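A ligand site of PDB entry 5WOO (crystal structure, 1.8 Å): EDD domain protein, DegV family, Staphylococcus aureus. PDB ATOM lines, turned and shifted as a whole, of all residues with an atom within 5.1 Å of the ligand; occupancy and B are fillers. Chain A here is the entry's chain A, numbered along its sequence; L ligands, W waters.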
ATOM      1  N   LEU A  34      17.056  -0.144 -10.107  1.00  0.00           N
ATOM      2  CA  LEU A  34      17.431  -1.024  -9.010  1.00  0.00           C
ATOM      3  C   LEU A  34      17.690  -0.165  -7.757  1.00  0.00           C
ATOM      4  O   LEU A  34      17.727   1.063  -7.821  1.00  0.00           O
ATOM      5  CB  LEU A  34      18.663  -1.865  -9.383  1.00  0.00           C
ATOM      6  CG  LEU A  34      18.413  -3.003 -10.390  1.00  0.00           C
ATOM      7  CD1 LEU A  34      18.445  -2.526 -11.859  1.00  0.00           C
ATOM      8  CD2 LEU A  34      19.433  -4.138 -10.163  1.00  0.00           C
ATOM      9  N   THR A  68      21.338  -5.233  -2.378  1.00  0.00           N
ATOM     10  CA  THR A  68      20.737  -4.613  -3.551  1.00  0.00           C
ATOM     11  C   THR A  68      19.471  -5.370  -3.913  1.00  0.00           C
ATOM     12  O   THR A  68      19.247  -6.498  -3.487  1.00  0.00           O
ATOM     13  CB  THR A  68      21.697  -4.583  -4.747  1.00  0.00           C
ATOM     14  OG1 THR A  68      22.002  -5.920  -5.159  1.00  0.00           O
ATOM     15  CG2 THR A  68      23.013  -3.853  -4.392  1.00  0.00           C
ATOM     16  N   SER A  69      18.628  -4.703  -4.706  1.00  0.00           N
ATOM     17  CA  SER A  69      17.370  -5.288  -5.163  1.00  0.00           C
ATOM     18  C   SER A  69      17.144  -4.926  -6.625  1.00  0.00           C
ATOM     19  O   SER A  69      17.281  -3.767  -7.024  1.00  0.00           O
ATOM     20  CB  SER A  69      16.178  -4.784  -4.338  1.00  0.00           C
ATOM     21  OG  SER A  69      16.326  -5.143  -2.969  1.00  0.00           O
ATOM     22  N   GLN A  70      16.791  -5.933  -7.414  1.00  0.00           N
ATOM     23  CA  GLN A  70      16.347  -5.775  -8.796  1.00  0.00           C
ATOM     24  C   GLN A  70      15.097  -4.905  -8.811  1.00  0.00           C
ATOM     25  O   GLN A  70      14.485  -4.678  -7.766  1.00  0.00           O
ATOM     26  CB  GLN A  70      16.051  -7.137  -9.398  1.00  0.00           C
ATOM     27  CG  GLN A  70      14.846  -7.790  -8.721  1.00  0.00           C
ATOM     28  CD  GLN A  70      14.466  -9.109  -9.336  1.00  0.00           C
ATOM     29  OE1 GLN A  70      13.469  -9.210 -10.042  1.00  0.00           O
ATOM     30  NE2 GLN A  70      15.267 -10.124  -9.086  1.00  0.00           N
ATOM     31  N   LEU A  96      20.371  -6.155 -17.316  1.00  0.00           N
ATOM     32  CA  LEU A  96      21.524  -6.732 -16.618  1.00  0.00           C
ATOM     33  C   LEU A  96      21.591  -8.242 -16.822  1.00  0.00           C
ATOM     34  O   LEU A  96      20.566  -8.915 -16.946  1.00  0.00           O
ATOM     35  CB  LEU A  96      21.360  -6.414 -15.126  1.00  0.00           C
ATOM     36  CG  LEU A  96      22.416  -6.751 -14.096  1.00  0.00           C
ATOM     37  CD1 LEU A  96      23.671  -5.980 -14.431  1.00  0.00           C
ATOM     38  CD2 LEU A  96      21.865  -6.336 -12.749  1.00  0.00           C
ATOM     39  N   ILE A 100      23.600 -12.763 -12.920  1.00  0.00           N
ATOM     40  CA  ILE A 100      23.900 -12.040 -11.695  1.00  0.00           C
ATOM     41  C   ILE A 100      22.679 -11.356 -11.099  1.00  0.00           C
ATOM     42  O   ILE A 100      22.772 -10.794 -10.009  1.00  0.00           O
ATOM     43  CB  ILE A 100      25.027 -11.001 -11.913  1.00  0.00           C
ATOM     44  CG1 ILE A 100      24.564  -9.829 -12.801  1.00  0.00           C
ATOM     45  CG2 ILE A 100      26.259 -11.686 -12.475  1.00  0.00           C
ATOM     46  CD1 ILE A 100      25.729  -8.853 -13.194  1.00  0.00           C
ATOM     47  N   SER A 101      21.532 -11.407 -11.763  1.00  0.00           N
ATOM     48  CA  SER A 101      20.377 -10.701 -11.243  1.00  0.00           C
ATOM     49  C   SER A 101      19.111 -11.302 -11.835  1.00  0.00           C
ATOM     50  O   SER A 101      19.113 -11.787 -12.964  1.00  0.00           O
ATOM     51  CB  SER A 101      20.464  -9.213 -11.588  1.00  0.00           C
ATOM     52  OG  SER A 101      19.295  -8.512 -11.216  1.00  0.00           O
ATOM     53  N   GLY A 102      18.022 -11.206 -11.069  1.00  0.00           N
ATOM     54  CA  GLY A 102      16.685 -11.567 -11.540  1.00  0.00           C
ATOM     55  C   GLY A 102      15.979 -10.505 -12.356  1.00  0.00           C
ATOM     56  O   GLY A 102      14.835 -10.723 -12.768  1.00  0.00           O
ATOM     57  N   LEU A 126      25.790  -8.928 -19.383  1.00  0.00           N
ATOM     58  CA  LEU A 126      26.842  -8.106 -18.769  1.00  0.00           C
ATOM     59  C   LEU A 126      26.214  -7.025 -17.909  1.00  0.00           C
ATOM     60  O   LEU A 126      25.124  -7.238 -17.345  1.00  0.00           O
ATOM     61  CB  LEU A 126      27.775  -7.539 -19.846  1.00  0.00           C
ATOM     62  CG  LEU A 126      29.168  -8.013 -19.408  1.00  0.00           C
ATOM     63  CD1 LEU A 126      30.096  -8.211 -20.566  1.00  0.00           C
ATOM     64  CD2 LEU A 126      29.755  -7.033 -18.381  1.00  0.00           C
ATOM     65  N   ALA A 127      26.860  -5.875 -17.790  1.00  0.00           N
ATOM     66  CA  ALA A 127      26.406  -4.840 -16.863  1.00  0.00           C
ATOM     67  C   ALA A 127      27.112  -3.528 -17.197  1.00  0.00           C
ATOM     68  O   ALA A 127      28.028  -3.478 -18.022  1.00  0.00           O
ATOM     69  CB  ALA A 127      26.670  -5.267 -15.421  1.00  0.00           C
ATOM     70  N   ALA A 128      26.646  -2.445 -16.554  1.00  0.00           N
ATOM     71  CA  ALA A 128      27.290  -1.138 -16.697  1.00  0.00           C
ATOM     72  C   ALA A 128      27.242  -0.691 -18.156  1.00  0.00           C
ATOM     73  O   ALA A 128      26.350  -1.098 -18.911  1.00  0.00           O
ATOM     74  CB  ALA A 128      28.741  -1.179 -16.127  1.00  0.00           C
ATOM     75  N   ALA A 164      34.093  -8.449 -20.717  1.00  0.00           N
ATOM     76  CA  ALA A 164      34.779  -7.531 -19.817  1.00  0.00           C
ATOM     77  C   ALA A 164      35.639  -8.315 -18.842  1.00  0.00           C
ATOM     78  O   ALA A 164      35.286  -9.425 -18.429  1.00  0.00           O
ATOM     79  CB  ALA A 164      33.789  -6.651 -19.040  1.00  0.00           C
ATOM     80  N   TYR A 165      36.767  -7.711 -18.472  1.00  0.00           N
ATOM     81  CA  TYR A 165      37.612  -8.151 -17.372  1.00  0.00           C
ATOM     82  C   TYR A 165      37.559  -7.084 -16.288  1.00  0.00           C
ATOM     83  O   TYR A 165      37.232  -5.923 -16.551  1.00  0.00           O
ATOM     84  CB  TYR A 165      39.044  -8.391 -17.859  1.00  0.00           C
ATOM     85  CG  TYR A 165      39.192  -9.586 -18.781  1.00  0.00           C
ATOM     86  CD1 TYR A 165      38.620  -9.594 -20.049  1.00  0.00           C
ATOM     87  CD2 TYR A 165      39.905 -10.722 -18.386  1.00  0.00           C
ATOM     88  CE1 TYR A 165      38.726 -10.684 -20.880  1.00  0.00           C
ATOM     89  CE2 TYR A 165      40.025 -11.824 -19.234  1.00  0.00           C
ATOM     90  CZ  TYR A 165      39.432 -11.789 -20.477  1.00  0.00           C
ATOM     91  OH  TYR A 165      39.535 -12.878 -21.331  1.00  0.00           O
ATOM     92  N   LEU A 166      37.852  -7.470 -15.045  1.00  0.00           N
ATOM     93  CA  LEU A 166      37.780  -6.491 -13.975  1.00  0.00           C
ATOM     94  C   LEU A 166      38.666  -6.918 -12.823  1.00  0.00           C
ATOM     95  O   LEU A 166      39.026  -8.101 -12.697  1.00  0.00           O
ATOM     96  CB  LEU A 166      36.352  -6.272 -13.477  1.00  0.00           C
ATOM     97  CG  LEU A 166      35.666  -7.520 -12.911  1.00  0.00           C
ATOM     98  CD1 LEU A 166      34.747  -7.172 -11.743  1.00  0.00           C
ATOM     99  CD2 LEU A 166      34.890  -8.230 -14.024  1.00  0.00           C
ATOM    100  N   LEU A 174      31.868  -9.503  -3.338  1.00  0.00           N
ATOM    101  CA  LEU A 174      31.341 -10.462  -4.308  1.00  0.00           C
ATOM    102  C   LEU A 174      31.015 -11.792  -3.646  1.00  0.00           C
ATOM    103  O   LEU A 174      30.010 -12.434  -3.982  1.00  0.00           O
ATOM    104  CB  LEU A 174      32.340 -10.660  -5.457  1.00  0.00           C
ATOM    105  CG  LEU A 174      32.397  -9.578  -6.538  1.00  0.00           C
ATOM    106  CD1 LEU A 174      33.650  -9.766  -7.383  1.00  0.00           C
ATOM    107  CD2 LEU A 174      31.119  -9.607  -7.402  1.00  0.00           C
ATOM    108  N   ARG A 179      28.034 -13.385  -6.018  1.00  0.00           N
ATOM    109  CA  ARG A 179      28.166 -13.024  -7.417  1.00  0.00           C
ATOM    110  C   ARG A 179      29.530 -13.363  -8.013  1.00  0.00           C
ATOM    111  O   ARG A 179      29.804 -12.996  -9.157  1.00  0.00           O
ATOM    112  CB  ARG A 179      27.886 -11.537  -7.642  1.00  0.00           C
ATOM    113  CG  ARG A 179      26.460 -11.249  -8.137  1.00  0.00           C
ATOM    114  CD  ARG A 179      25.451 -11.684  -7.092  1.00  0.00           C
ATOM    115  NE  ARG A 179      24.102 -11.277  -7.497  1.00  0.00           N
ATOM    116  CZ  ARG A 179      23.063 -11.219  -6.666  1.00  0.00           C
ATOM    117  NH1 ARG A 179      23.220 -11.537  -5.388  1.00  0.00           N
ATOM    118  NH2 ARG A 179      21.882 -10.825  -7.119  1.00  0.00           N
ATOM    119  N   PHE A 199      33.891 -11.789 -17.172  1.00  0.00           N
ATOM    120  CA  PHE A 199      32.565 -12.327 -17.429  1.00  0.00           C
ATOM    121  C   PHE A 199      32.666 -13.495 -18.395  1.00  0.00           C
ATOM    122  O   PHE A 199      33.430 -13.462 -19.363  1.00  0.00           O
ATOM    123  CB  PHE A 199      31.643 -11.270 -18.023  1.00  0.00           C
ATOM    124  CG  PHE A 199      30.888 -10.487 -17.005  1.00  0.00           C
ATOM    125  CD1 PHE A 199      31.524  -9.478 -16.297  1.00  0.00           C
ATOM    126  CD2 PHE A 199      29.549 -10.760 -16.754  1.00  0.00           C
ATOM    127  CE1 PHE A 199      30.836  -8.733 -15.354  1.00  0.00           C
ATOM    128  CE2 PHE A 199      28.850 -10.025 -15.814  1.00  0.00           C
ATOM    129  CZ  PHE A 199      29.486  -9.015 -15.106  1.00  0.00           C
ATOM    130  N   ILE A 204      30.425 -14.095 -13.370  1.00  0.00           N
ATOM    131  CA  ILE A 204      31.752 -13.568 -13.049  1.00  0.00           C
ATOM    132  C   ILE A 204      32.606 -14.706 -12.514  1.00  0.00           C
ATOM    133  O   ILE A 204      32.239 -15.350 -11.523  1.00  0.00           O
ATOM    134  CB  ILE A 204      31.646 -12.421 -12.033  1.00  0.00           C
ATOM    135  CG1 ILE A 204      30.817 -11.286 -12.624  1.00  0.00           C
ATOM    136  CG2 ILE A 204      33.054 -11.938 -11.607  1.00  0.00           C
ATOM    137  CD1 ILE A 204      30.553 -10.136 -11.639  1.00  0.00           C
ATOM    138  N   ILE A 239      35.704   1.186 -17.103  1.00  0.00           N
ATOM    139  CA  ILE A 239      34.559   1.348 -16.209  1.00  0.00           C
ATOM    140  C   ILE A 239      35.138   1.434 -14.806  1.00  0.00           C
ATOM    141  O   ILE A 239      35.574   0.434 -14.238  1.00  0.00           O
ATOM    142  CB  ILE A 239      33.564   0.196 -16.347  1.00  0.00           C
ATOM    143  CG1 ILE A 239      33.132   0.071 -17.814  1.00  0.00           C
ATOM    144  CG2 ILE A 239      32.356   0.438 -15.450  1.00  0.00           C
ATOM    145  CD1 ILE A 239      32.071  -0.999 -18.054  1.00  0.00           C
ATOM    146  N   PHE A 269      31.026   2.920 -12.494  1.00  0.00           N
ATOM    147  CA  PHE A 269      30.005   2.081 -11.859  1.00  0.00           C
ATOM    148  C   PHE A 269      29.083   2.930 -11.001  1.00  0.00           C
ATOM    149  O   PHE A 269      29.519   3.846 -10.302  1.00  0.00           O
ATOM    150  CB  PHE A 269      30.655   1.035 -10.945  1.00  0.00           C
ATOM    151  CG  PHE A 269      31.564   0.084 -11.650  1.00  0.00           C
ATOM    152  CD1 PHE A 269      31.075  -0.790 -12.601  1.00  0.00           C
ATOM    153  CD2 PHE A 269      32.921   0.031 -11.321  1.00  0.00           C
ATOM    154  CE1 PHE A 269      31.910  -1.682 -13.233  1.00  0.00           C
ATOM    155  CE2 PHE A 269      33.758  -0.841 -11.953  1.00  0.00           C
ATOM    156  CZ  PHE A 269      33.253  -1.712 -12.919  1.00  0.00           C
ATOM    157  N   VAL A 272      24.666   0.192  -7.276  1.00  0.00           N
ATOM    158  CA  VAL A 272      24.313  -1.215  -7.179  1.00  0.00           C
ATOM    159  C   VAL A 272      25.500  -2.100  -7.522  1.00  0.00           C
ATOM    160  O   VAL A 272      25.789  -3.072  -6.818  1.00  0.00           O
ATOM    161  CB  VAL A 272      23.084  -1.523  -8.067  1.00  0.00           C
ATOM    162  CG1 VAL A 272      22.955  -3.036  -8.280  1.00  0.00           C
ATOM    163  CG2 VAL A 272      21.821  -0.946  -7.407  1.00  0.00           C
ATOM    164  N   VAL A 273      26.228  -1.788  -8.597  1.00  0.00           N
ATOM    165  CA  VAL A 273      27.413  -2.582  -8.922  1.00  0.00           C
ATOM    166  C   VAL A 273      28.516  -2.370  -7.889  1.00  0.00           C
ATOM    167  O   VAL A 273      29.220  -3.313  -7.511  1.00  0.00           O
ATOM    168  CB  VAL A 273      27.893  -2.259 -10.352  1.00  0.00           C
ATOM    169  CG1 VAL A 273      29.320  -2.775 -10.576  1.00  0.00           C
ATOM    170  CG2 VAL A 273      26.911  -2.851 -11.377  1.00  0.00           C
ATOM    171  N   HIS A 276      28.368  -4.627  -4.867  1.00  0.00           N
ATOM    172  CA  HIS A 276      28.840  -5.992  -5.059  1.00  0.00           C
ATOM    173  C   HIS A 276      30.336  -6.064  -5.263  1.00  0.00           C
ATOM    174  O   HIS A 276      30.946  -7.065  -4.877  1.00  0.00           O
ATOM    175  CB  HIS A 276      28.116  -6.627  -6.253  1.00  0.00           C
ATOM    176  CG  HIS A 276      26.662  -6.894  -6.001  1.00  0.00           C
ATOM    177  ND1 HIS A 276      26.196  -8.130  -5.584  1.00  0.00           N
ATOM    178  CD2 HIS A 276      25.574  -6.096  -6.075  1.00  0.00           C
ATOM    179  CE1 HIS A 276      24.887  -8.072  -5.424  1.00  0.00           C
ATOM    180  NE2 HIS A 276      24.483  -6.850  -5.718  1.00  0.00           N
ATOM    181  N   LEU A 277      30.962  -5.030  -5.840  1.00  0.00           N
ATOM    182  CA  LEU A 277      32.404  -5.054  -6.049  1.00  0.00           C
ATOM    183  C   LEU A 277      33.166  -4.597  -4.821  1.00  0.00           C
ATOM    184  O   LEU A 277      34.255  -5.106  -4.556  1.00  0.00           O
ATOM    185  CB  LEU A 277      32.788  -4.166  -7.246  1.00  0.00           C
ATOM    186  CG  LEU A 277      32.178  -4.582  -8.589  1.00  0.00           C
ATOM    187  CD1 LEU A 277      32.777  -3.745  -9.719  1.00  0.00           C
ATOM    188  CD2 LEU A 277      32.418  -6.064  -8.840  1.00  0.00           C
ATOM    189  N   GLY A 283      36.949  -2.018 -14.286  1.00  0.00           N
ATOM    190  CA  GLY A 283      36.671  -2.918 -15.377  1.00  0.00           C
ATOM    191  C   GLY A 283      37.175  -2.378 -16.702  1.00  0.00           C
ATOM    192  O   GLY A 283      37.315  -1.162 -16.884  1.00  0.00           O
HETATM  193  C1  LIG L   1      20.349  -7.315  -7.981  1.00  0.00           C
HETATM  194  O1  LIG L   1      20.104  -7.112  -6.756  1.00  0.00           O
HETATM  195  O2  LIG L   1      19.621  -8.121  -8.624  1.00  0.00           O
HETATM  196  C2  LIG L   1      21.514  -6.575  -8.659  1.00  0.00           C
HETATM  197  C3  LIG L   1      22.747  -7.491  -8.761  1.00  0.00           C
HETATM  198  C4  LIG L   1      23.959  -6.672  -9.222  1.00  0.00           C
HETATM  199  C5  LIG L   1      25.163  -7.604  -9.342  1.00  0.00           C
HETATM  200  C6  LIG L   1      26.419  -6.840  -9.800  1.00  0.00           C
HETATM  201  C7  LIG L   1      27.635  -7.786  -9.855  1.00  0.00           C
HETATM  202  C8  LIG L   1      28.953  -7.034 -10.162  1.00  0.00           C
HETATM  203  C9  LIG L   1      28.933  -6.509 -11.604  1.00  0.00           C
HETATM  204  C10 LIG L   1      30.282  -5.951 -12.055  1.00  0.00           C
HETATM  205  C11 LIG L   1      30.115  -5.347 -13.454  1.00  0.00           C
HETATM  206  C12 LIG L   1      31.479  -5.181 -14.090  1.00  0.00           C
HETATM  207  C13 LIG L   1      31.329  -4.689 -15.535  1.00  0.00           C
HETATM  208  C14 LIG L   1      32.740  -4.400 -16.047  1.00  0.00           C
HETATM  209  O   HOH W   1      21.334  -8.979  -4.577  1.00  0.00           O
HETATM  210  O   HOH W   2      17.810 -10.280  -8.246  1.00  0.00           O
HETATM  211  O   HOH W   3      17.409  -8.633  -6.364  1.00  0.00           O
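An oxygen (O1) of the ligand sits at hydrogen-bond distance from the backbone NH of Ser 69, at 3.5 Å.
NH2 of Arg 179 lies within salt-bridge range of O2 of the ligand.
O1 of the ligand sits at hydrogen-bond distance from OG1 of Thr 68 (2.8 Å).
The side-chain hydroxyl (OG) of Ser 101 is in hydrogen-bond range of an oxygen (O2) of the ligand, at 2.6 Å.
OE1 of Gln 70 lies close to O of Gly 102.
N of Phe 199 sits at hydrogen-bond distance from O of Ala 164, at 3.0 Å.
The backbone NH of Arg 179 sits at hydrogen-bond distance from the backbone carbonyl oxygen of Leu 174 (3.0 Å).
OG1 of Thr 68 is in hydrogen-bond range of NE2 of His 276.
The backbone carbonyl oxygen of His 276 is in hydrogen-bond range of the backbone NH of Leu 174, 3.0 Å away.
The backbone carbonyl oxygen of Ile 100 is in hydrogen-bond range of the guanidinium group of Arg 179 (2.9 Å).
Merely in contact with the ligand: Leu 34 (3.5 Å), Gln 70 (3.6 Å), Ile 100 (3.5 Å), Ala 127 (3.97 Å), Ala 164 (3.9 Å), Phe 199 (3.8 Å), Ile 204 (3.8 Å), Phe 269 (3.6 Å), Val 272 (3.8 Å), Val 273 (3.6 Å), His 276 (3.5 Å) and Leu 277 (3.8 Å).
Hydrophobic or aromatic side chains within 4 Å of the ligand: Leu 34, Ile 100, Ala 127, Ala 164, Phe 199, Ile 204, Phe 269, Val 272, Val 273, His 276 and Leu 277.
Within 4 Å of the ligand: Leu 34, Thr 68, Ser 69, Gln 70, Ile 100, Ser 101, Ala 127, Ala 164, Arg 179, Phe 199, Ile 204, Phe 269, Val 272, Val 273, His 276 and Leu 277.
Water W2 lies within hydrogen-bond range of the side-chain amide nitrogen of Gln 70 (2.7 Å), an oxygen (O2) of the ligand (2.8 Å) and the backbone NH of Gly 102 (3.0 Å).
Water W3 lies within hydrogen-bond range of N of Gln 70 (3.0 Å) and O1 of the ligand (3.1 Å).
Water W1 lies within hydrogen-bond range of an oxygen (O1) of the ligand, the side-chain hydroxyl of Thr 68 and the guanidinium group of Arg 179.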
